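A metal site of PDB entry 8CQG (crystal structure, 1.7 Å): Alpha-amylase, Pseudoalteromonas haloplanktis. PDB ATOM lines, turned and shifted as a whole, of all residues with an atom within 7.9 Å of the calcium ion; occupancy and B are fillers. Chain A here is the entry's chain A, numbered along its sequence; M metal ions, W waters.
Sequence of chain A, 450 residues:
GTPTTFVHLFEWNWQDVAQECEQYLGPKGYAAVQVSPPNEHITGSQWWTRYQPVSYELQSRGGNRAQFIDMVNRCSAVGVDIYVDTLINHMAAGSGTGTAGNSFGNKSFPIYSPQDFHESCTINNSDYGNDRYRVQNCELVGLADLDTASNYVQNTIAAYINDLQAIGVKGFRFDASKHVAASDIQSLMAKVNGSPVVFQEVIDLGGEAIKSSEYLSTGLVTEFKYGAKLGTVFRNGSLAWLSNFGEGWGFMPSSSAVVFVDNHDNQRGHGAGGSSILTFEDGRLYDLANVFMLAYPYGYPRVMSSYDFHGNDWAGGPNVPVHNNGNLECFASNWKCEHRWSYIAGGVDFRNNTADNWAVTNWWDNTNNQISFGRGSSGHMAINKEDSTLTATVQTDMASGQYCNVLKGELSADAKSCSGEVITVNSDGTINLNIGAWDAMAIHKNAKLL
ND1 of His 179 sits at hydrogen-bond distance from O of Val 135 (3.0 Å).
The backbone carbonyl oxygen of Asn 89 is in hydrogen-bond range of the backbone NH of Leu 146 (3.1 Å).
The side-chain amide nitrogen (ND2) of Asn 89 sits at hydrogen-bond distance from a ring nitrogen (ND1) of His 90.
O of Lys 178 lies within hydrogen-bond range of NE2 of Gln 136, at 3.1 Å.
The backbone NH of His 118 sits at hydrogen-bond distance from the backbone carbonyl oxygen of Asp 145.
Water W2 bridges O of Asn 89 (2.7 Å) and O of Leu 146 (2.7 Å).
The calcium ion is bound by water W1 (2.2 Å), the backbone carbonyl oxygen (O) of His 179 (2.3 Å), the side-chain amide oxygen (OD1) of Asn 89 (2.4 Å), water W3 (2.5 Å), the backbone carbonyl oxygen (O) of Gln 136 (2.5 Å), water W2 (2.5 Å), the side-chain carboxylate (OD2) of Asp 145 (2.5 Å) and the side-chain carboxylate (OD1) of Asp 145 (2.6 Å).
The calcium ion has eight donor atoms within binding distance.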
ATOM      1  N   ILE A  88       3.982  32.133   3.565  1.00  0.00           N
ATOM      2  CA  ILE A  88       3.424  33.084   2.603  1.00  0.00           C
ATOM      3  C   ILE A  88       2.110  32.623   1.987  1.00  0.00           C
ATOM      4  O   ILE A  88       1.446  33.428   1.324  1.00  0.00           O
ATOM      5  CB  ILE A  88       4.401  33.384   1.436  1.00  0.00           C
ATOM      6  CG1 ILE A  88       4.720  32.122   0.643  1.00  0.00           C
ATOM      7  CG2 ILE A  88       5.682  34.031   1.962  1.00  0.00           C
ATOM      8  CD1 ILE A  88       5.418  32.400  -0.692  1.00  0.00           C
ATOM      9  N   ASN A  89       1.729  31.374   2.172  1.00  0.00           N
ATOM     10  CA  ASN A  89       0.614  30.823   1.414  1.00  0.00           C
ATOM     11  C   ASN A  89      -0.710  30.873   2.162  1.00  0.00           C
ATOM     12  O   ASN A  89      -1.765  30.913   1.506  1.00  0.00           O
ATOM     13  CB  ASN A  89       0.895  29.374   1.029  1.00  0.00           C
ATOM     14  CG  ASN A  89      -0.257  28.742   0.256  1.00  0.00           C
ATOM     15  OD1 ASN A  89      -0.563  29.147  -0.863  1.00  0.00           O
ATOM     16  ND2 ASN A  89      -0.858  27.737   0.838  1.00  0.00           N
ATOM     17  N   HIS A  90      -0.709  30.845   3.488  1.00  0.00           N
ATOM     18  CA  HIS A  90      -1.943  30.491   4.164  1.00  0.00           C
ATOM     19  C   HIS A  90      -1.925  30.908   5.626  1.00  0.00           C
ATOM     20  O   HIS A  90      -0.899  31.328   6.175  1.00  0.00           O
ATOM     21  CB  HIS A  90      -2.195  28.982   4.056  1.00  0.00           C
ATOM     22  CG  HIS A  90      -1.058  28.169   4.596  1.00  0.00           C
ATOM     23  ND1 HIS A  90      -0.102  27.602   3.790  1.00  0.00           N
ATOM     24  CD2 HIS A  90      -0.713  27.859   5.871  1.00  0.00           C
ATOM     25  CE1 HIS A  90       0.787  26.972   4.542  1.00  0.00           C
ATOM     26  NE2 HIS A  90       0.440  27.116   5.810  1.00  0.00           N
ATOM     27  N   HIS A 118      -8.664  33.432  -0.869  1.00  0.00           N
ATOM     28  CA  HIS A 118      -9.350  32.833  -2.008  1.00  0.00           C
ATOM     29  C   HIS A 118     -10.621  32.146  -1.534  1.00  0.00           C
ATOM     30  O   HIS A 118     -10.702  31.657  -0.398  1.00  0.00           O
ATOM     31  CB  HIS A 118      -8.476  31.816  -2.731  1.00  0.00           C
ATOM     32  CG  HIS A 118      -7.267  32.421  -3.370  1.00  0.00           C
ATOM     33  ND1 HIS A 118      -6.031  31.821  -3.336  1.00  0.00           N
ATOM     34  CD2 HIS A 118      -7.111  33.590  -4.031  1.00  0.00           C
ATOM     35  CE1 HIS A 118      -5.166  32.578  -3.977  1.00  0.00           C
ATOM     36  NE2 HIS A 118      -5.781  33.657  -4.412  1.00  0.00           N
ATOM     37  N   ILE A 123      -7.711  21.318  -2.439  1.00  0.00           N
ATOM     38  CA  ILE A 123      -6.723  20.722  -3.337  1.00  0.00           C
ATOM     39  C   ILE A 123      -6.881  19.210  -3.256  1.00  0.00           C
ATOM     40  O   ILE A 123      -6.744  18.625  -2.179  1.00  0.00           O
ATOM     41  CB  ILE A 123      -5.298  21.152  -2.958  1.00  0.00           C
ATOM     42  CG1 ILE A 123      -5.163  22.668  -3.036  1.00  0.00           C
ATOM     43  CG2 ILE A 123      -4.286  20.471  -3.911  1.00  0.00           C
ATOM     44  CD1 ILE A 123      -3.778  23.207  -2.592  1.00  0.00           C
ATOM     45  N   TYR A 133      -4.335  26.005 -11.323  1.00  0.00           N
ATOM     46  CA  TYR A 133      -5.200  26.972 -10.655  1.00  0.00           C
ATOM     47  C   TYR A 133      -5.598  26.482  -9.282  1.00  0.00           C
ATOM     48  O   TYR A 133      -5.537  27.231  -8.298  1.00  0.00           O
ATOM     49  CB  TYR A 133      -6.450  27.248 -11.510  1.00  0.00           C
ATOM     50  CG  TYR A 133      -7.403  28.219 -10.846  1.00  0.00           C
ATOM     51  CD1 TYR A 133      -7.267  29.577 -11.049  1.00  0.00           C
ATOM     52  CD2 TYR A 133      -8.421  27.778 -10.001  1.00  0.00           C
ATOM     53  CE1 TYR A 133      -8.127  30.480 -10.446  1.00  0.00           C
ATOM     54  CE2 TYR A 133      -9.269  28.675  -9.394  1.00  0.00           C
ATOM     55  CZ  TYR A 133      -9.113  30.024  -9.623  1.00  0.00           C
ATOM     56  OH  TYR A 133      -9.956  30.938  -9.030  1.00  0.00           O
ATOM     57  N   ARG A 134      -6.036  25.222  -9.192  1.00  0.00           N
ATOM     58  CA  ARG A 134      -6.496  24.672  -7.924  1.00  0.00           C
ATOM     59  C   ARG A 134      -5.340  24.492  -6.935  1.00  0.00           C
ATOM     60  O   ARG A 134      -5.494  24.769  -5.748  1.00  0.00           O
ATOM     61  CB  ARG A 134      -7.203  23.338  -8.164  1.00  0.00           C
ATOM     62  CG  ARG A 134      -8.577  23.469  -8.815  1.00  0.00           C
ATOM     63  CD  ARG A 134      -9.265  22.108  -8.925  1.00  0.00           C
ATOM     64  NE  ARG A 134      -9.709  21.607  -7.630  1.00  0.00           N
ATOM     65  CZ  ARG A 134     -10.842  21.949  -7.040  1.00  0.00           C
ATOM     66  NH1 ARG A 134     -11.674  22.833  -7.570  1.00  0.00           N
ATOM     67  NH2 ARG A 134     -11.160  21.384  -5.875  1.00  0.00           N
ATOM     68  N   VAL A 135      -4.192  24.010  -7.409  1.00  0.00           N
ATOM     69  CA  VAL A 135      -3.027  23.899  -6.518  1.00  0.00           C
ATOM     70  C   VAL A 135      -2.729  25.227  -5.841  1.00  0.00           C
ATOM     71  O   VAL A 135      -2.368  25.281  -4.657  1.00  0.00           O
ATOM     72  CB  VAL A 135      -1.789  23.390  -7.287  1.00  0.00           C
ATOM     73  CG1 VAL A 135      -0.585  23.380  -6.358  1.00  0.00           C
ATOM     74  CG2 VAL A 135      -2.040  22.006  -7.866  1.00  0.00           C
ATOM     75  N   GLN A 136      -2.911  26.326  -6.562  1.00  0.00           N
ATOM     76  CA  GLN A 136      -2.482  27.627  -6.076  1.00  0.00           C
ATOM     77  C   GLN A 136      -3.598  28.479  -5.478  1.00  0.00           C
ATOM     78  O   GLN A 136      -3.313  29.435  -4.759  1.00  0.00           O
ATOM     79  CB  GLN A 136      -1.782  28.390  -7.192  1.00  0.00           C
ATOM     80  CG  GLN A 136      -0.549  27.602  -7.720  1.00  0.00           C
ATOM     81  CD  GLN A 136       0.323  28.378  -8.708  1.00  0.00           C
ATOM     82  OE1 GLN A 136      -0.171  29.189  -9.502  1.00  0.00           O
ATOM     83  NE2 GLN A 136       1.644  28.104  -8.680  1.00  0.00           N
ATOM     84  N   ASN A 137      -4.866  28.149  -5.751  1.00  0.00           N
ATOM     85  CA  ASN A 137      -5.976  28.937  -5.219  1.00  0.00           C
ATOM     86  C   ASN A 137      -6.836  28.197  -4.214  1.00  0.00           C
ATOM     87  O   ASN A 137      -7.510  28.848  -3.406  1.00  0.00           O
ATOM     88  CB  ASN A 137      -6.840  29.452  -6.382  1.00  0.00           C
ATOM     89  CG  ASN A 137      -6.126  30.512  -7.199  1.00  0.00           C
ATOM     90  OD1 ASN A 137      -6.249  31.699  -6.924  1.00  0.00           O
ATOM     91  ND2 ASN A 137      -5.357  30.093  -8.189  1.00  0.00           N
ATOM     92  N   CYS A 138      -6.779  26.867  -4.179  1.00  0.00           N
ATOM     93  CA  CYS A 138      -7.537  26.080  -3.229  1.00  0.00           C
ATOM     94  C   CYS A 138      -6.717  25.841  -1.956  1.00  0.00           C
ATOM     95  O   CYS A 138      -5.553  26.241  -1.840  1.00  0.00           O
ATOM     96  CB  CYS A 138      -7.979  24.755  -3.838  1.00  0.00           C
ATOM     97  SG  CYS A 138      -9.165  24.981  -5.198  1.00  0.00           S
ATOM     98  N   GLU A 139      -7.349  25.130  -1.024  1.00  0.00           N
ATOM     99  CA  GLU A 139      -6.826  24.996   0.334  1.00  0.00           C
ATOM    100  C   GLU A 139      -5.997  23.734   0.460  1.00  0.00           C
ATOM    101  O   GLU A 139      -6.454  22.628   0.189  1.00  0.00           O
ATOM    102  CB  GLU A 139      -7.977  24.972   1.349  1.00  0.00           C
ATOM    103  CG  GLU A 139      -8.663  26.306   1.430  1.00  0.00           C
ATOM    104  CD  GLU A 139      -9.815  26.308   2.411  1.00  0.00           C
ATOM    105  OE1 GLU A 139     -10.243  25.206   2.821  1.00  0.00           O
ATOM    106  OE2 GLU A 139     -10.266  27.415   2.786  1.00  0.00           O
ATOM    107  N   LEU A 140      -4.764  23.917   0.916  1.00  0.00           N
ATOM    108  CA  LEU A 140      -3.904  22.816   1.302  1.00  0.00           C
ATOM    109  C   LEU A 140      -4.308  22.324   2.690  1.00  0.00           C
ATOM    110  O   LEU A 140      -4.248  23.090   3.652  1.00  0.00           O
ATOM    111  CB  LEU A 140      -2.454  23.298   1.252  1.00  0.00           C
ATOM    112  CG  LEU A 140      -1.351  22.338   1.665  1.00  0.00           C
ATOM    113  CD1 LEU A 140      -1.347  21.135   0.766  1.00  0.00           C
ATOM    114  CD2 LEU A 140      -0.008  23.093   1.610  1.00  0.00           C
ATOM    115  N   LEU A 143      -6.032  24.631   5.174  1.00  0.00           N
ATOM    116  CA  LEU A 143      -5.474  25.923   5.554  1.00  0.00           C
ATOM    117  C   LEU A 143      -6.098  27.025   4.722  1.00  0.00           C
ATOM    118  O   LEU A 143      -6.155  26.935   3.487  1.00  0.00           O
ATOM    119  CB  LEU A 143      -3.950  25.886   5.355  1.00  0.00           C
ATOM    120  CG  LEU A 143      -3.262  24.766   6.109  1.00  0.00           C
ATOM    121  CD1 LEU A 143      -1.900  24.427   5.481  1.00  0.00           C
ATOM    122  CD2 LEU A 143      -3.093  25.087   7.567  1.00  0.00           C
ATOM    123  N   ALA A 144      -6.543  28.094   5.376  1.00  0.00           N
ATOM    124  CA  ALA A 144      -7.124  29.223   4.660  1.00  0.00           C
ATOM    125  C   ALA A 144      -6.108  29.800   3.680  1.00  0.00           C
ATOM    126  O   ALA A 144      -5.022  30.229   4.085  1.00  0.00           O
ATOM    127  CB  ALA A 144      -7.589  30.296   5.635  1.00  0.00           C
ATOM    128  N   ASP A 145      -6.475  29.842   2.409  1.00  0.00           N
ATOM    129  CA  ASP A 145      -5.542  30.177   1.331  1.00  0.00           C
ATOM    130  C   ASP A 145      -5.580  31.671   1.066  1.00  0.00           C
ATOM    131  O   ASP A 145      -6.543  32.201   0.488  1.00  0.00           O
ATOM    132  CB  ASP A 145      -5.882  29.368   0.071  1.00  0.00           C
ATOM    133  CG  ASP A 145      -4.684  29.245  -0.860  1.00  0.00           C
ATOM    134  OD1 ASP A 145      -3.669  28.653  -0.436  1.00  0.00           O
ATOM    135  OD2 ASP A 145      -4.761  29.745  -2.002  1.00  0.00           O
ATOM    136  N   LEU A 146      -4.511  32.357   1.467  1.00  0.00           N
ATOM    137  CA  LEU A 146      -4.439  33.804   1.296  1.00  0.00           C
ATOM    138  C   LEU A 146      -4.525  34.190  -0.177  1.00  0.00           C
ATOM    139  O   LEU A 146      -4.027  33.488  -1.052  1.00  0.00           O
ATOM    140  CB  LEU A 146      -3.131  34.324   1.894  1.00  0.00           C
ATOM    141  CG  LEU A 146      -3.145  34.487   3.415  1.00  0.00           C
ATOM    142  CD1 LEU A 146      -1.708  34.621   3.952  1.00  0.00           C
ATOM    143  CD2 LEU A 146      -3.993  35.677   3.843  1.00  0.00           C
ATOM    144  N   ASP A 147      -5.185  35.322  -0.439  1.00  0.00           N
ATOM    145  CA  ASP A 147      -5.220  35.907  -1.782  1.00  0.00           C
ATOM    146  C   ASP A 147      -3.921  36.666  -1.975  1.00  0.00           C
ATOM    147  O   ASP A 147      -3.811  37.858  -1.693  1.00  0.00           O
ATOM    148  CB  ASP A 147      -6.431  36.821  -1.963  1.00  0.00           C
ATOM    149  CG  ASP A 147      -6.486  37.415  -3.352  1.00  0.00           C
ATOM    150  OD1 ASP A 147      -5.704  36.970  -4.221  1.00  0.00           O
ATOM    151  OD2 ASP A 147      -7.302  38.344  -3.559  1.00  0.00           O
ATOM    152  N   THR A 148      -2.896  35.923  -2.428  1.00  0.00           N
ATOM    153  CA  THR A 148      -1.573  36.492  -2.560  1.00  0.00           C
ATOM    154  C   THR A 148      -1.446  37.423  -3.757  1.00  0.00           C
ATOM    155  O   THR A 148      -0.374  37.985  -3.967  1.00  0.00           O
ATOM    156  CB  THR A 148      -0.547  35.341  -2.638  1.00  0.00           C
ATOM    157  OG1 THR A 148      -1.027  34.337  -3.520  1.00  0.00           O
ATOM    158  CG2 THR A 148      -0.376  34.711  -1.252  1.00  0.00           C
ATOM    159  N   ALA A 176       5.777  26.512   1.248  1.00  0.00           N
ATOM    160  CA  ALA A 176       4.652  26.160   0.373  1.00  0.00           C
ATOM    161  C   ALA A 176       4.580  27.032  -0.889  1.00  0.00           C
ATOM    162  O   ALA A 176       3.511  27.408  -1.358  1.00  0.00           O
ATOM    163  CB  ALA A 176       3.318  26.226   1.152  1.00  0.00           C
ATOM    164  N   SER A 177       5.737  27.303  -1.483  1.00  0.00           N
ATOM    165  CA  SER A 177       5.780  28.258  -2.590  1.00  0.00           C
ATOM    166  C   SER A 177       5.088  27.721  -3.842  1.00  0.00           C
ATOM    167  O   SER A 177       4.599  28.507  -4.664  1.00  0.00           O
ATOM    168  CB  SER A 177       7.220  28.652  -2.898  1.00  0.00           C
ATOM    169  OG  SER A 177       7.737  29.543  -1.926  1.00  0.00           O
ATOM    170  N   LYS A 178       5.021  26.398  -4.002  1.00  0.00           N
ATOM    171  CA  LYS A 178       4.303  25.823  -5.131  1.00  0.00           C
ATOM    172  C   LYS A 178       2.856  26.275  -5.155  1.00  0.00           C
ATOM    173  O   LYS A 178       2.249  26.379  -6.224  1.00  0.00           O
ATOM    174  CB  LYS A 178       4.357  24.295  -5.067  1.00  0.00           C
ATOM    175  CG  LYS A 178       3.667  23.608  -6.253  1.00  0.00           C
ATOM    176  CD  LYS A 178       4.290  22.254  -6.604  1.00  0.00           C
ATOM    177  CE  LYS A 178       3.810  21.157  -5.723  1.00  0.00           C
ATOM    178  NZ  LYS A 178       4.597  19.917  -6.019  1.00  0.00           N
ATOM    179  N   HIS A 179       2.292  26.533  -3.981  1.00  0.00           N
ATOM    180  CA  HIS A 179       0.897  26.889  -3.805  1.00  0.00           C
ATOM    181  C   HIS A 179       0.652  28.371  -3.986  1.00  0.00           C
ATOM    182  O   HIS A 179      -0.469  28.842  -3.767  1.00  0.00           O
ATOM    183  CB  HIS A 179       0.441  26.399  -2.431  1.00  0.00           C
ATOM    184  CG  HIS A 179       0.538  24.911  -2.286  1.00  0.00           C
ATOM    185  ND1 HIS A 179      -0.430  24.063  -2.792  1.00  0.00           N
ATOM    186  CD2 HIS A 179       1.494  24.121  -1.760  1.00  0.00           C
ATOM    187  CE1 HIS A 179      -0.074  22.812  -2.566  1.00  0.00           C
ATOM    188  NE2 HIS A 179       1.093  22.817  -1.933  1.00  0.00           N
ATOM    189  N   VAL A 180       1.684  29.113  -4.378  1.00  0.00           N
ATOM    190  CA  VAL A 180       1.615  30.534  -4.661  1.00  0.00           C
ATOM    191  C   VAL A 180       2.156  30.751  -6.064  1.00  0.00           C
ATOM    192  O   VAL A 180       3.293  30.368  -6.350  1.00  0.00           O
ATOM    193  CB  VAL A 180       2.402  31.382  -3.649  1.00  0.00           C
ATOM    194  CG1 VAL A 180       2.303  32.844  -4.007  1.00  0.00           C
ATOM    195  CG2 VAL A 180       1.910  31.124  -2.208  1.00  0.00           C
ATOM    196  N   ALA A 181       1.361  31.377  -6.935  1.00  0.00           N
ATOM    197  CA  ALA A 181       1.875  31.739  -8.256  1.00  0.00           C
ATOM    198  C   ALA A 181       3.198  32.480  -8.145  1.00  0.00           C
ATOM    199  O   ALA A 181       3.349  33.396  -7.330  1.00  0.00           O
ATOM    200  CB  ALA A 181       0.849  32.603  -9.006  1.00  0.00           C
ATOM    201  N   ASP A 184       2.764  36.113  -8.092  1.00  0.00           N
ATOM    202  CA  ASP A 184       2.466  36.674  -6.780  1.00  0.00           C
ATOM    203  C   ASP A 184       3.739  36.878  -5.958  1.00  0.00           C
ATOM    204  O   ASP A 184       3.897  37.902  -5.274  1.00  0.00           O
ATOM    205  CB  ASP A 184       1.478  35.761  -6.032  1.00  0.00           C
ATOM    206  CG  ASP A 184       0.064  35.807  -6.613  1.00  0.00           C
ATOM    207  OD1 ASP A 184      -0.155  36.584  -7.572  1.00  0.00           O
ATOM    208  OD2 ASP A 184      -0.817  35.057  -6.116  1.00  0.00           O
HETATM  209 CA    CA M   1      -2.312  29.510  -2.512  1.00  0.00          CA
HETATM  210  O   HOH W   1      -2.927  27.366  -2.650  1.00  0.00           O
HETATM  211  O   HOH W   2      -2.236  31.510  -1.041  1.00  0.00           O
HETATM  212  O   HOH W   3      -1.897  31.602  -3.718  1.00  0.00           O
